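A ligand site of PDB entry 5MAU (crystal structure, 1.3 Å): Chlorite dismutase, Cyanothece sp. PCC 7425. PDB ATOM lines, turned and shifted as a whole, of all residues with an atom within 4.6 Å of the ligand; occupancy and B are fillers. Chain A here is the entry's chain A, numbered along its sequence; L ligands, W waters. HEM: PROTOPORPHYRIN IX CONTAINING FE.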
ATOM      1  N   ASN A  64       2.547  23.361   2.247  1.00  0.00           N
ATOM      2  CA  ASN A  64       1.969  24.435   3.047  1.00  0.00           C
ATOM      3  C   ASN A  64       0.469  24.538   2.813  1.00  0.00           C
ATOM      4  O   ASN A  64      -0.082  24.009   1.840  1.00  0.00           O
ATOM      5  CB  ASN A  64       2.609  25.790   2.709  1.00  0.00           C
ATOM      6  CG  ASN A  64       2.423  26.168   1.242  1.00  0.00           C
ATOM      7  OD1 ASN A  64       3.138  25.663   0.391  1.00  0.00           O
ATOM      8  ND2 ASN A  64       1.491  27.052   0.943  1.00  0.00           N
ATOM      9  N   ILE A  65      -0.172  25.183   3.759  1.00  0.00           N
ATOM     10  CA  ILE A  65      -1.602  25.477   3.744  1.00  0.00           C
ATOM     11  C   ILE A  65      -1.941  26.361   2.559  1.00  0.00           C
ATOM     12  O   ILE A  65      -1.274  27.378   2.298  1.00  0.00           O
ATOM     13  CB  ILE A  65      -2.018  26.069   5.101  1.00  0.00           C
ATOM     14  CG1 ILE A  65      -1.950  24.998   6.203  1.00  0.00           C
ATOM     15  CG2 ILE A  65      -3.356  26.828   5.067  1.00  0.00           C
ATOM     16  CD1 ILE A  65      -3.032  23.937   6.061  1.00  0.00           C
ATOM     17  N   ARG A  66      -3.058  26.030   1.898  1.00  0.00           N
ATOM     18  CA  ARG A  66      -3.509  26.700   0.691  1.00  0.00           C
ATOM     19  C   ARG A  66      -4.805  27.485   0.916  1.00  0.00           C
ATOM     20  O   ARG A  66      -5.103  28.388   0.116  1.00  0.00           O
ATOM     21  CB  ARG A  66      -3.720  25.652  -0.451  1.00  0.00           C
ATOM     22  CG  ARG A  66      -2.572  24.744  -0.653  1.00  0.00           C
ATOM     23  CD  ARG A  66      -1.264  25.503  -0.941  1.00  0.00           C
ATOM     24  NE  ARG A  66      -0.173  24.639  -1.164  1.00  0.00           N
ATOM     25  CZ  ARG A  66       0.109  23.991  -2.342  1.00  0.00           C
ATOM     26  NH1 ARG A  66      -0.652  24.258  -3.425  1.00  0.00           N
ATOM     27  NH2 ARG A  66       1.107  23.138  -2.498  1.00  0.00           N
ATOM     28  N   TYR A  67      -5.620  27.110   1.919  1.00  0.00           N
ATOM     29  CA  TYR A  67      -6.954  27.676   2.100  1.00  0.00           C
ATOM     30  C   TYR A  67      -7.283  28.072   3.542  1.00  0.00           C
ATOM     31  O   TYR A  67      -7.956  29.072   3.788  1.00  0.00           O
ATOM     32  CB  TYR A  67      -8.074  26.718   1.598  1.00  0.00           C
ATOM     33  CG  TYR A  67      -8.002  26.530   0.106  1.00  0.00           C
ATOM     34  CD1 TYR A  67      -8.281  27.561  -0.767  1.00  0.00           C
ATOM     35  CD2 TYR A  67      -7.619  25.303  -0.468  1.00  0.00           C
ATOM     36  CE1 TYR A  67      -8.167  27.396  -2.138  1.00  0.00           C
ATOM     37  CE2 TYR A  67      -7.500  25.135  -1.855  1.00  0.00           C
ATOM     38  CZ  TYR A  67      -7.797  26.210  -2.673  1.00  0.00           C
ATOM     39  OH  TYR A  67      -7.666  26.057  -4.035  1.00  0.00           O
ATOM     40  N   ALA A  68      -6.875  27.220   4.475  1.00  0.00           N
ATOM     41  CA  ALA A  68      -7.316  27.419   5.863  1.00  0.00           C
ATOM     42  C   ALA A  68      -6.798  28.724   6.438  1.00  0.00           C
ATOM     43  O   ALA A  68      -5.632  29.086   6.230  1.00  0.00           O
ATOM     44  CB  ALA A  68      -6.807  26.293   6.716  1.00  0.00           C
ATOM     45  N   LEU A  76      -8.639  23.367  14.278  1.00  0.00           N
ATOM     46  CA  LEU A  76      -8.113  22.070  13.904  1.00  0.00           C
ATOM     47  C   LEU A  76      -7.053  21.620  14.895  1.00  0.00           C
ATOM     48  O   LEU A  76      -7.020  20.469  15.310  1.00  0.00           O
ATOM     49  CB  LEU A  76      -7.524  22.147  12.485  1.00  0.00           C
ATOM     50  CG  LEU A  76      -8.553  22.299  11.388  1.00  0.00           C
ATOM     51  CD1 LEU A  76      -7.910  22.813  10.076  1.00  0.00           C
ATOM     52  CD2 LEU A  76      -9.224  20.931  11.054  1.00  0.00           C
ATOM     53  N   ILE A  94      -7.504   7.967  -0.485  1.00  0.00           N
ATOM     54  CA  ILE A  94      -8.474   8.504  -1.448  1.00  0.00           C
ATOM     55  C   ILE A  94      -7.781   9.439  -2.422  1.00  0.00           C
ATOM     56  O   ILE A  94      -7.642  10.641  -2.124  1.00  0.00           O
ATOM     57  CB  ILE A  94      -9.722   9.125  -0.810  1.00  0.00           C
ATOM     58  CG1 ILE A  94     -10.350   8.162   0.227  1.00  0.00           C
ATOM     59  CG2 ILE A  94     -10.726   9.571  -1.917  1.00  0.00           C
ATOM     60  CD1 ILE A  94     -11.531   8.731   0.918  1.00  0.00           C
ATOM     61  N   ILE A  96      -7.614  11.872  -5.506  1.00  0.00           N
ATOM     62  CA  ILE A  96      -8.615  12.790  -6.031  1.00  0.00           C
ATOM     63  C   ILE A  96      -8.005  13.585  -7.174  1.00  0.00           C
ATOM     64  O   ILE A  96      -6.879  14.085  -7.032  1.00  0.00           O
ATOM     65  CB  ILE A  96      -9.153  13.727  -4.944  1.00  0.00           C
ATOM     66  CG1 ILE A  96      -9.995  12.828  -4.029  1.00  0.00           C
ATOM     67  CG2 ILE A  96      -9.937  14.924  -5.467  1.00  0.00           C
ATOM     68  CD1 ILE A  96     -10.255  13.355  -2.775  1.00  0.00           C
ATOM     69  N   LYS A  98      -9.169  17.019  -9.537  1.00  0.00           N
ATOM     70  CA  LYS A  98     -10.124  18.077  -9.819  1.00  0.00           C
ATOM     71  C   LYS A  98      -9.979  18.547 -11.253  1.00  0.00           C
ATOM     72  O   LYS A  98      -8.968  18.322 -11.896  1.00  0.00           O
ATOM     73  CB  LYS A  98      -9.932  19.241  -8.824  1.00  0.00           C
ATOM     74  CG  LYS A  98     -10.343  18.880  -7.411  1.00  0.00           C
ATOM     75  CD  LYS A  98     -10.240  20.105  -6.440  1.00  0.00           C
ATOM     76  CE  LYS A  98     -10.697  19.755  -5.046  1.00  0.00           C
ATOM     77  NZ  LYS A  98     -10.853  20.999  -4.196  1.00  0.00           N
ATOM     78  N   TRP A 102     -11.645  23.994 -12.264  1.00  0.00           N
ATOM     79  CA  TRP A 102     -11.235  24.308 -10.898  1.00  0.00           C
ATOM     80  C   TRP A 102      -9.891  25.040 -10.892  1.00  0.00           C
ATOM     81  O   TRP A 102      -9.740  26.121 -10.274  1.00  0.00           O
ATOM     82  CB  TRP A 102     -11.154  23.018 -10.092  1.00  0.00           C
ATOM     83  CG  TRP A 102     -10.559  23.242  -8.723  1.00  0.00           C
ATOM     84  CD1 TRP A 102      -9.267  22.989  -8.351  1.00  0.00           C
ATOM     85  CD2 TRP A 102     -11.224  23.754  -7.560  1.00  0.00           C
ATOM     86  NE1 TRP A 102      -9.097  23.342  -7.020  1.00  0.00           N
ATOM     87  CE2 TRP A 102     -10.270  23.821  -6.512  1.00  0.00           C
ATOM     88  CE3 TRP A 102     -12.520  24.190  -7.286  1.00  0.00           C
ATOM     89  CZ2 TRP A 102     -10.588  24.239  -5.239  1.00  0.00           C
ATOM     90  CZ3 TRP A 102     -12.811  24.636  -6.046  1.00  0.00           C
ATOM     91  CH2 TRP A 102     -11.848  24.655  -5.031  1.00  0.00           C
ATOM     92  N   PHE A 114     -14.566  26.278  -1.535  1.00  0.00           N
ATOM     93  CA  PHE A 114     -14.060  25.293  -0.589  1.00  0.00           C
ATOM     94  C   PHE A 114     -14.726  25.439   0.769  1.00  0.00           C
ATOM     95  O   PHE A 114     -15.178  24.456   1.365  1.00  0.00           O
ATOM     96  CB  PHE A 114     -12.539  25.482  -0.487  1.00  0.00           C
ATOM     97  CG  PHE A 114     -11.858  24.587   0.466  1.00  0.00           C
ATOM     98  CD1 PHE A 114     -11.560  23.273   0.136  1.00  0.00           C
ATOM     99  CD2 PHE A 114     -11.501  25.030   1.710  1.00  0.00           C
ATOM    100  CE1 PHE A 114     -10.941  22.438   0.999  1.00  0.00           C
ATOM    101  CE2 PHE A 114     -10.844  24.171   2.605  1.00  0.00           C
ATOM    102  CZ  PHE A 114     -10.573  22.872   2.223  1.00  0.00           C
ATOM    103  N   HIS A 120     -15.944  22.803   3.904  1.00  0.00           N
ATOM    104  CA  HIS A 120     -15.079  21.627   3.988  1.00  0.00           C
ATOM    105  C   HIS A 120     -14.509  21.458   5.388  1.00  0.00           C
ATOM    106  O   HIS A 120     -14.567  20.377   5.957  1.00  0.00           O
ATOM    107  CB  HIS A 120     -13.963  21.715   2.924  1.00  0.00           C
ATOM    108  CG  HIS A 120     -13.089  20.504   2.805  1.00  0.00           C
ATOM    109  ND1 HIS A 120     -12.939  19.858   1.606  1.00  0.00           N
ATOM    110  CD2 HIS A 120     -12.314  19.832   3.696  1.00  0.00           C
ATOM    111  CE1 HIS A 120     -12.046  18.867   1.755  1.00  0.00           C
ATOM    112  NE2 HIS A 120     -11.711  18.797   3.041  1.00  0.00           N
ATOM    113  N   THR A 121     -13.898  22.520   5.948  1.00  0.00           N
ATOM    114  CA  THR A 121     -13.249  22.405   7.246  1.00  0.00           C
ATOM    115  C   THR A 121     -14.287  22.275   8.365  1.00  0.00           C
ATOM    116  O   THR A 121     -14.123  21.464   9.281  1.00  0.00           O
ATOM    117  CB  THR A 121     -12.341  23.606   7.482  1.00  0.00           C
ATOM    118  OG1 THR A 121     -11.316  23.582   6.495  1.00  0.00           O
ATOM    119  CG2 THR A 121     -11.682  23.527   8.813  1.00  0.00           C
ATOM    120  N   GLY A 124     -15.662  18.744   8.160  1.00  0.00           N
ATOM    121  CA  GLY A 124     -14.637  17.803   8.575  1.00  0.00           C
ATOM    122  C   GLY A 124     -14.418  17.823  10.072  1.00  0.00           C
ATOM    123  O   GLY A 124     -14.182  16.780  10.684  1.00  0.00           O
ATOM    124  N   LEU A 125     -14.400  19.023  10.670  1.00  0.00           N
ATOM    125  CA  LEU A 125     -14.188  19.112  12.108  1.00  0.00           C
ATOM    126  C   LEU A 125     -15.209  18.292  12.908  1.00  0.00           C
ATOM    127  O   LEU A 125     -14.911  17.866  14.043  1.00  0.00           O
ATOM    128  CB  LEU A 125     -14.286  20.579  12.569  1.00  0.00           C
ATOM    129  CG  LEU A 125     -12.983  21.353  12.445  1.00  0.00           C
ATOM    130  CD1 LEU A 125     -13.266  22.854  12.466  1.00  0.00           C
ATOM    131  CD2 LEU A 125     -12.053  20.993  13.535  1.00  0.00           C
ATOM    132  N   LEU A 128     -13.708  14.884  13.941  1.00  0.00           N
ATOM    133  CA  LEU A 128     -12.528  14.834  14.772  1.00  0.00           C
ATOM    134  C   LEU A 128     -12.983  14.795  16.226  1.00  0.00           C
ATOM    135  O   LEU A 128     -13.984  15.434  16.568  1.00  0.00           O
ATOM    136  CB  LEU A 128     -11.672  16.103  14.547  1.00  0.00           C
ATOM    137  CG  LEU A 128     -10.744  15.984  13.334  1.00  0.00           C
ATOM    138  CD1 LEU A 128     -11.333  15.397  12.083  1.00  0.00           C
ATOM    139  CD2 LEU A 128     -10.049  17.312  13.068  1.00  0.00           C
ATOM    140  N   VAL A 131     -11.289  10.774  13.443  1.00  0.00           N
ATOM    141  CA  VAL A 131     -10.583  10.583  12.162  1.00  0.00           C
ATOM    142  C   VAL A 131      -9.292  11.419  12.153  1.00  0.00           C
ATOM    143  O   VAL A 131      -9.345  12.652  12.321  1.00  0.00           O
ATOM    144  CB  VAL A 131     -11.467  10.957  10.986  1.00  0.00           C
ATOM    145  CG1 VAL A 131     -10.702  10.803   9.653  1.00  0.00           C
ATOM    146  CG2 VAL A 131     -12.729  10.061  10.962  1.00  0.00           C
ATOM    147  N   ARG A 133      -5.867  12.424   9.705  1.00  0.00           N
ATOM    148  CA  ARG A 133      -5.732  12.651   8.266  1.00  0.00           C
ATOM    149  C   ARG A 133      -4.357  13.121   7.891  1.00  0.00           C
ATOM    150  O   ARG A 133      -3.641  13.736   8.690  1.00  0.00           O
ATOM    151  CB  ARG A 133      -6.811  13.641   7.772  1.00  0.00           C
ATOM    152  CG  ARG A 133      -6.540  15.140   8.169  1.00  0.00           C
ATOM    153  CD  ARG A 133      -7.731  16.049   7.941  1.00  0.00           C
ATOM    154  NE  ARG A 133      -7.224  17.438   8.069  1.00  0.00           N
ATOM    155  CZ  ARG A 133      -6.938  18.005   9.224  1.00  0.00           C
ATOM    156  NH1 ARG A 133      -7.239  17.437  10.388  1.00  0.00           N
ATOM    157  NH2 ARG A 133      -6.355  19.209   9.223  1.00  0.00           N
ATOM    158  N   LEU A 135      -2.874  15.169   4.153  1.00  0.00           N
ATOM    159  CA  LEU A 135      -3.073  15.653   2.801  1.00  0.00           C
ATOM    160  C   LEU A 135      -1.754  15.682   2.059  1.00  0.00           C
ATOM    161  O   LEU A 135      -0.805  16.360   2.504  1.00  0.00           O
ATOM    162  CB  LEU A 135      -3.719  17.044   2.849  1.00  0.00           C
ATOM    163  CG  LEU A 135      -3.860  17.781   1.511  1.00  0.00           C
ATOM    164  CD1 LEU A 135      -4.835  16.973   0.580  1.00  0.00           C
ATOM    165  CD2 LEU A 135      -4.340  19.172   1.756  1.00  0.00           C
ATOM    166  N   PHE A 147      -4.360  14.981  -5.697  1.00  0.00           N
ATOM    167  CA  PHE A 147      -4.168  14.847  -4.263  1.00  0.00           C
ATOM    168  C   PHE A 147      -4.181  13.390  -3.882  1.00  0.00           C
ATOM    169  O   PHE A 147      -4.887  12.591  -4.503  1.00  0.00           O
ATOM    170  CB  PHE A 147      -5.236  15.552  -3.455  1.00  0.00           C
ATOM    171  CG  PHE A 147      -5.498  16.979  -3.857  1.00  0.00           C
ATOM    172  CD1 PHE A 147      -4.688  18.008  -3.352  1.00  0.00           C
ATOM    173  CD2 PHE A 147      -6.508  17.332  -4.707  1.00  0.00           C
ATOM    174  CE1 PHE A 147      -4.905  19.298  -3.748  1.00  0.00           C
ATOM    175  CE2 PHE A 147      -6.759  18.664  -5.045  1.00  0.00           C
ATOM    176  CZ  PHE A 147      -5.961  19.663  -4.533  1.00  0.00           C
ATOM    177  N   THR A 149      -5.243  11.717  -0.411  1.00  0.00           N
ATOM    178  CA  THR A 149      -5.803  11.984   0.907  1.00  0.00           C
ATOM    179  C   THR A 149      -5.744  10.729   1.722  1.00  0.00           C
ATOM    180  O   THR A 149      -6.039   9.635   1.208  1.00  0.00           O
ATOM    181  CB  THR A 149      -7.172  12.681   0.881  1.00  0.00           C
ATOM    182  OG1 THR A 149      -8.165  11.779   0.330  1.00  0.00           O
ATOM    183  CG2 THR A 149      -7.128  13.927   0.075  1.00  0.00           C
ATOM    184  N   PHE A 151      -6.769   8.861   5.529  1.00  0.00           N
ATOM    185  CA  PHE A 151      -7.561   8.911   6.755  1.00  0.00           C
ATOM    186  C   PHE A 151      -7.332   7.637   7.548  1.00  0.00           C
ATOM    187  O   PHE A 151      -7.235   6.550   6.974  1.00  0.00           O
ATOM    188  CB  PHE A 151      -9.057   9.099   6.421  1.00  0.00           C
ATOM    189  CG  PHE A 151      -9.263  10.294   5.537  1.00  0.00           C
ATOM    190  CD1 PHE A 151      -9.312  11.554   6.092  1.00  0.00           C
ATOM    191  CD2 PHE A 151      -9.247  10.154   4.162  1.00  0.00           C
ATOM    192  CE1 PHE A 151      -9.409  12.653   5.254  1.00  0.00           C
ATOM    193  CE2 PHE A 151      -9.323  11.272   3.327  1.00  0.00           C
ATOM    194  CZ  PHE A 151      -9.393  12.532   3.901  1.00  0.00           C
ATOM    195  N   PHE A 161     -17.229   7.927   9.337  1.00  0.00           N
ATOM    196  CA  PHE A 161     -16.428   8.245   8.157  1.00  0.00           C
ATOM    197  C   PHE A 161     -17.235   8.076   6.890  1.00  0.00           C
ATOM    198  O   PHE A 161     -17.143   8.890   5.952  1.00  0.00           O
ATOM    199  CB  PHE A 161     -15.122   7.464   8.144  1.00  0.00           C
ATOM    200  CG  PHE A 161     -14.209   7.899   7.060  1.00  0.00           C
ATOM    201  CD1 PHE A 161     -13.461   9.051   7.179  1.00  0.00           C
ATOM    202  CD2 PHE A 161     -14.046   7.160   5.895  1.00  0.00           C
ATOM    203  CE1 PHE A 161     -12.664   9.473   6.134  1.00  0.00           C
ATOM    204  CE2 PHE A 161     -13.204   7.590   4.890  1.00  0.00           C
ATOM    205  CZ  PHE A 161     -12.527   8.745   5.016  1.00  0.00           C
ATOM    206  N   LEU A 164     -19.402  11.016   6.455  1.00  0.00           N
ATOM    207  CA  LEU A 164     -18.610  12.156   5.986  1.00  0.00           C
ATOM    208  C   LEU A 164     -18.408  12.113   4.482  1.00  0.00           C
ATOM    209  O   LEU A 164     -18.598  13.126   3.783  1.00  0.00           O
ATOM    210  CB  LEU A 164     -17.233  12.186   6.711  1.00  0.00           C
ATOM    211  CG  LEU A 164     -16.233  13.219   6.177  1.00  0.00           C
ATOM    212  CD1 LEU A 164     -16.777  14.628   6.266  1.00  0.00           C
ATOM    213  CD2 LEU A 164     -14.917  13.109   6.948  1.00  0.00           C
ATOM    214  N   LEU A 165     -18.028  10.946   3.959  1.00  0.00           N
ATOM    215  CA  LEU A 165     -17.793  10.835   2.532  1.00  0.00           C
ATOM    216  C   LEU A 165     -19.032  11.252   1.767  1.00  0.00           C
ATOM    217  O   LEU A 165     -18.930  11.919   0.732  1.00  0.00           O
ATOM    218  CB  LEU A 165     -17.409   9.409   2.148  1.00  0.00           C
ATOM    219  CG  LEU A 165     -16.049   8.908   2.613  1.00  0.00           C
ATOM    220  CD1 LEU A 165     -15.847   7.507   2.217  1.00  0.00           C
ATOM    221  CD2 LEU A 165     -14.917   9.775   2.044  1.00  0.00           C
ATOM    222  N   MET A 168     -19.467  15.065   1.816  1.00  0.00           N
ATOM    223  CA  MET A 168     -18.548  15.805   0.954  1.00  0.00           C
ATOM    224  C   MET A 168     -18.878  15.608  -0.522  1.00  0.00           C
ATOM    225  O   MET A 168     -18.756  16.541  -1.318  1.00  0.00           O
ATOM    226  CB  MET A 168     -17.123  15.356   1.206  1.00  0.00           C
ATOM    227  CG  MET A 168     -16.765  15.733   2.609  1.00  0.00           C
ATOM    228  SD  MET A 168     -15.116  15.467   3.125  1.00  0.00           S
ATOM    229  CE  MET A 168     -14.306  16.519   1.965  1.00  0.00           C
ATOM    230  N   GLU A 173     -17.979  21.847  -3.874  1.00  0.00           N
ATOM    231  CA  GLU A 173     -16.607  21.534  -4.188  1.00  0.00           C
ATOM    232  C   GLU A 173     -16.505  20.250  -5.004  1.00  0.00           C
ATOM    233  O   GLU A 173     -15.689  20.134  -5.938  1.00  0.00           O
ATOM    234  CB  GLU A 173     -15.815  21.397  -2.900  1.00  0.00           C
ATOM    235  CG  GLU A 173     -14.359  20.925  -3.123  1.00  0.00           C
ATOM    236  CD  GLU A 173     -13.592  20.720  -1.832  1.00  0.00           C
ATOM    237  OE1 GLU A 173     -14.222  20.670  -0.744  1.00  0.00           O
ATOM    238  OE2 GLU A 173     -12.344  20.527  -1.923  1.00  0.00           O
ATOM    239  N   TRP A 174     -17.348  19.242  -4.686  1.00  0.00           N
ATOM    240  CA  TRP A 174     -17.242  17.977  -5.359  1.00  0.00           C
ATOM    241  C   TRP A 174     -17.785  18.014  -6.794  1.00  0.00           C
ATOM    242  O   TRP A 174     -17.550  17.072  -7.540  1.00  0.00           O
ATOM    243  CB  TRP A 174     -17.928  16.872  -4.527  1.00  0.00           C
ATOM    244  CG  TRP A 174     -16.884  15.846  -4.114  1.00  0.00           C
ATOM    245  CD1 TRP A 174     -16.675  14.614  -4.629  1.00  0.00           C
ATOM    246  CD2 TRP A 174     -15.868  16.019  -3.102  1.00  0.00           C
ATOM    247  NE1 TRP A 174     -15.610  13.998  -4.028  1.00  0.00           N
ATOM    248  CE2 TRP A 174     -15.095  14.851  -3.091  1.00  0.00           C
ATOM    249  CE3 TRP A 174     -15.522  17.070  -2.234  1.00  0.00           C
ATOM    250  CZ2 TRP A 174     -14.022  14.671  -2.231  1.00  0.00           C
ATOM    251  CZ3 TRP A 174     -14.410  16.893  -1.395  1.00  0.00           C
ATOM    252  CH2 TRP A 174     -13.682  15.710  -1.381  1.00  0.00           C
ATOM    253  N   GLU A 180     -11.821   9.834  -8.681  1.00  0.00           N
ATOM    254  CA  GLU A 180     -11.814   9.547  -7.265  1.00  0.00           C
ATOM    255  C   GLU A 180     -11.813   8.036  -7.071  1.00  0.00           C
ATOM    256  O   GLU A 180     -12.632   7.337  -7.721  1.00  0.00           O
ATOM    257  CB  GLU A 180     -12.978  10.172  -6.565  1.00  0.00           C
ATOM    258  CG  GLU A 180     -12.997   9.915  -5.081  1.00  0.00           C
ATOM    259  CD  GLU A 180     -13.918  10.820  -4.361  1.00  0.00           C
ATOM    260  OE1 GLU A 180     -14.798  11.425  -4.998  1.00  0.00           O
ATOM    261  OE2 GLU A 180     -13.722  11.035  -3.172  1.00  0.00           O
HETATM  262  CHA HEM L   1      -8.090  19.837   2.077  1.00  0.00           C
HETATM  263  CHB HEM L   1      -9.754  19.328   6.587  1.00  0.00           C
HETATM  264  CHC HEM L   1     -11.858  15.133   5.282  1.00  0.00           C
HETATM  265  CHD HEM L   1     -10.296  15.740   0.733  1.00  0.00           C
HETATM  266  C1A HEM L   1      -8.383  20.083   3.387  1.00  0.00           C
HETATM  267  C2A HEM L   1      -8.026  21.311   4.131  1.00  0.00           C
HETATM  268  C3A HEM L   1      -8.474  21.116   5.410  1.00  0.00           C
HETATM  269  C4A HEM L   1      -9.181  19.852   5.473  1.00  0.00           C
HETATM  270  CMA HEM L   1      -8.382  22.076   6.619  1.00  0.00           C
HETATM  271  CAA HEM L   1      -7.280  22.529   3.538  1.00  0.00           C
HETATM  272  CBA HEM L   1      -5.795  22.409   3.777  1.00  0.00           C
HETATM  273  CGA HEM L   1      -5.146  23.673   3.171  1.00  0.00           C
HETATM  274  O1A HEM L   1      -4.217  23.523   2.341  1.00  0.00           O
HETATM  275  O2A HEM L   1      -5.611  24.822   3.514  1.00  0.00           O
HETATM  276  C1B HEM L   1     -10.458  18.121   6.601  1.00  0.00           C
HETATM  277  C2B HEM L   1     -10.962  17.505   7.823  1.00  0.00           C
HETATM  278  C3B HEM L   1     -11.498  16.328   7.484  1.00  0.00           C
HETATM  279  C4B HEM L   1     -11.321  16.189   6.035  1.00  0.00           C
HETATM  280  CMB HEM L   1     -10.846  18.099   9.245  1.00  0.00           C
HETATM  281  CAB HEM L   1     -12.096  15.345   8.500  1.00  0.00           C
HETATM  282  CBB HEM L   1     -11.807  14.038   8.340  1.00  0.00           C
HETATM  283  C1C HEM L   1     -11.676  14.987   3.913  1.00  0.00           C
HETATM  284  C2C HEM L   1     -12.181  13.870   3.111  1.00  0.00           C
HETATM  285  C3C HEM L   1     -11.695  14.014   1.885  1.00  0.00           C
HETATM  286  C4C HEM L   1     -10.927  15.241   1.836  1.00  0.00           C
HETATM  287  CMC HEM L   1     -12.932  12.679   3.699  1.00  0.00           C
HETATM  288  CAC HEM L   1     -11.856  13.123   0.673  1.00  0.00           C
HETATM  289  CBC HEM L   1     -12.957  12.473   0.409  1.00  0.00           C
HETATM  290  C1D HEM L   1      -9.498  16.906   0.719  1.00  0.00           C
HETATM  291  C2D HEM L   1      -8.847  17.455  -0.446  1.00  0.00           C
HETATM  292  C3D HEM L   1      -8.201  18.582  -0.091  1.00  0.00           C
HETATM  293  C4D HEM L   1      -8.490  18.767   1.318  1.00  0.00           C
HETATM  294  CMD HEM L   1      -8.912  16.789  -1.833  1.00  0.00           C
HETATM  295  CAD HEM L   1      -7.426  19.525  -1.016  1.00  0.00           C
HETATM  296  CBD HEM L   1      -8.363  20.610  -1.489  1.00  0.00           C
HETATM  297  CGD HEM L   1      -7.698  21.548  -2.494  1.00  0.00           C
HETATM  298  O1D HEM L   1      -6.532  21.978  -2.255  1.00  0.00           O
HETATM  299  O2D HEM L   1      -8.345  21.882  -3.522  1.00  0.00           O
HETATM  300  NA  HEM L   1      -9.083  19.205   4.238  1.00  0.00           N
HETATM  301  NB  HEM L   1     -10.642  17.319   5.462  1.00  0.00           N
HETATM  302  NC  HEM L   1     -10.939  15.832   3.082  1.00  0.00           N
HETATM  303  ND  HEM L   1      -9.272  17.718   1.831  1.00  0.00           N
HETATM  304 FE   HEM L   1     -10.129  17.600   3.640  1.00  0.00          FE
HETATM  305  O   HOH W   1      -4.965  22.095  -0.127  1.00  0.00           O
HETATM  306  O   HOH W   2      -4.583  23.277  -3.793  1.00  0.00           O
HETATM  307  O   HOH W   3      -7.837  16.440   4.079  1.00  0.00           O
HETATM  308  O   HOH W   4      -6.247  18.332   5.448  1.00  0.00           O
HETATM  309  O   HOH W   5      -2.009  21.956   2.150  1.00  0.00           O
HETATM  310  O   HOH W   6      -7.078  23.702  -4.989  1.00  0.00           O
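N of Tyr 67 is in hydrogen-bond range of O2A of the ligand, at 2.8 Å. NE2 of His 120 is bound to FE of the ligand, at 2.1 Å. An oxygen (O2D) of the ligand lies within salt-bridge range of the side-chain amino group of Lys 98 (2.7 Å). O1A of the ligand sits at hydrogen-bond distance from N of Arg 66. N of Ala 68 lies within hydrogen-bond range of O2A of the ligand, at 2.9 Å.
The guanidinium group (NE) of Arg 66 lies within hydrogen-bond range of the backbone carbonyl oxygen (O) of Asn 64. A ring nitrogen (ND1) of His 120 sits at hydrogen-bond distance from the side-chain carboxylate (OE1) of Glu 173, at 2.8 Å. OG1 of Thr 149 lies within hydrogen-bond range of O of Ile 94. The backbone NH (N) of His 120 sits at hydrogen-bond distance from the backbone carbonyl oxygen (O) of Phe 114, 3.1 Å away. OE2 of Glu 173 is in salt-bridge range of NZ of Lys 98 (2.8 Å). N of Phe 147 sits at hydrogen-bond distance from O of Ile 96, at 3.0 Å. The side-chain carboxylate (OE1) of Glu 180 lies within hydrogen-bond range of the indole nitrogen (NE1) of Trp 174, 2.9 Å away.
Residues that only touch the ligand: Ile 65 (3.4 Å), Leu 76 (3.6 Å), Ile 96 (3.8 Å), Trp 102 (3.7 Å), Phe 114 (3.5 Å), Thr 121 (3.3 Å), Gly 124 (3.3 Å), Leu 125 (3.9 Å), Leu 128 (3.7 Å), Val 131 (3.7 Å), Arg 133 (3.5 Å), Leu 135 (3.8 Å), Phe 147 (3.3 Å), Thr 149 (3.7 Å), Phe 151 (3.2 Å), Leu 164 (3.5 Å), Leu 165 (3.7 Å), Met 168 (3.3 Å), Trp 174 (3.6 Å) and Glu 180 (3.9 Å). Hydrophobic or aromatic side chains that line the ligand: Ile 65, Tyr 67, Ala 68, Leu 76, Ile 96, Trp 102, Phe 114, His 120, Leu 128, Val 131, Leu 135, Phe 147, Phe 151, Leu 164, Leu 165, Met 168 and Trp 174. The nearest printed residue that does not touch the ligand is Glu 173 (4.01 Å).
Water W6 lies within hydrogen-bond range of the side-chain hydroxyl of Tyr 67, an oxygen (O2D) of the ligand and the indole nitrogen of Trp 102. Water W5 bridges an oxygen (O1A) of the ligand (2.7 Å) and the backbone carbonyl oxygen (O) of Asn 64 (2.8 Å).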
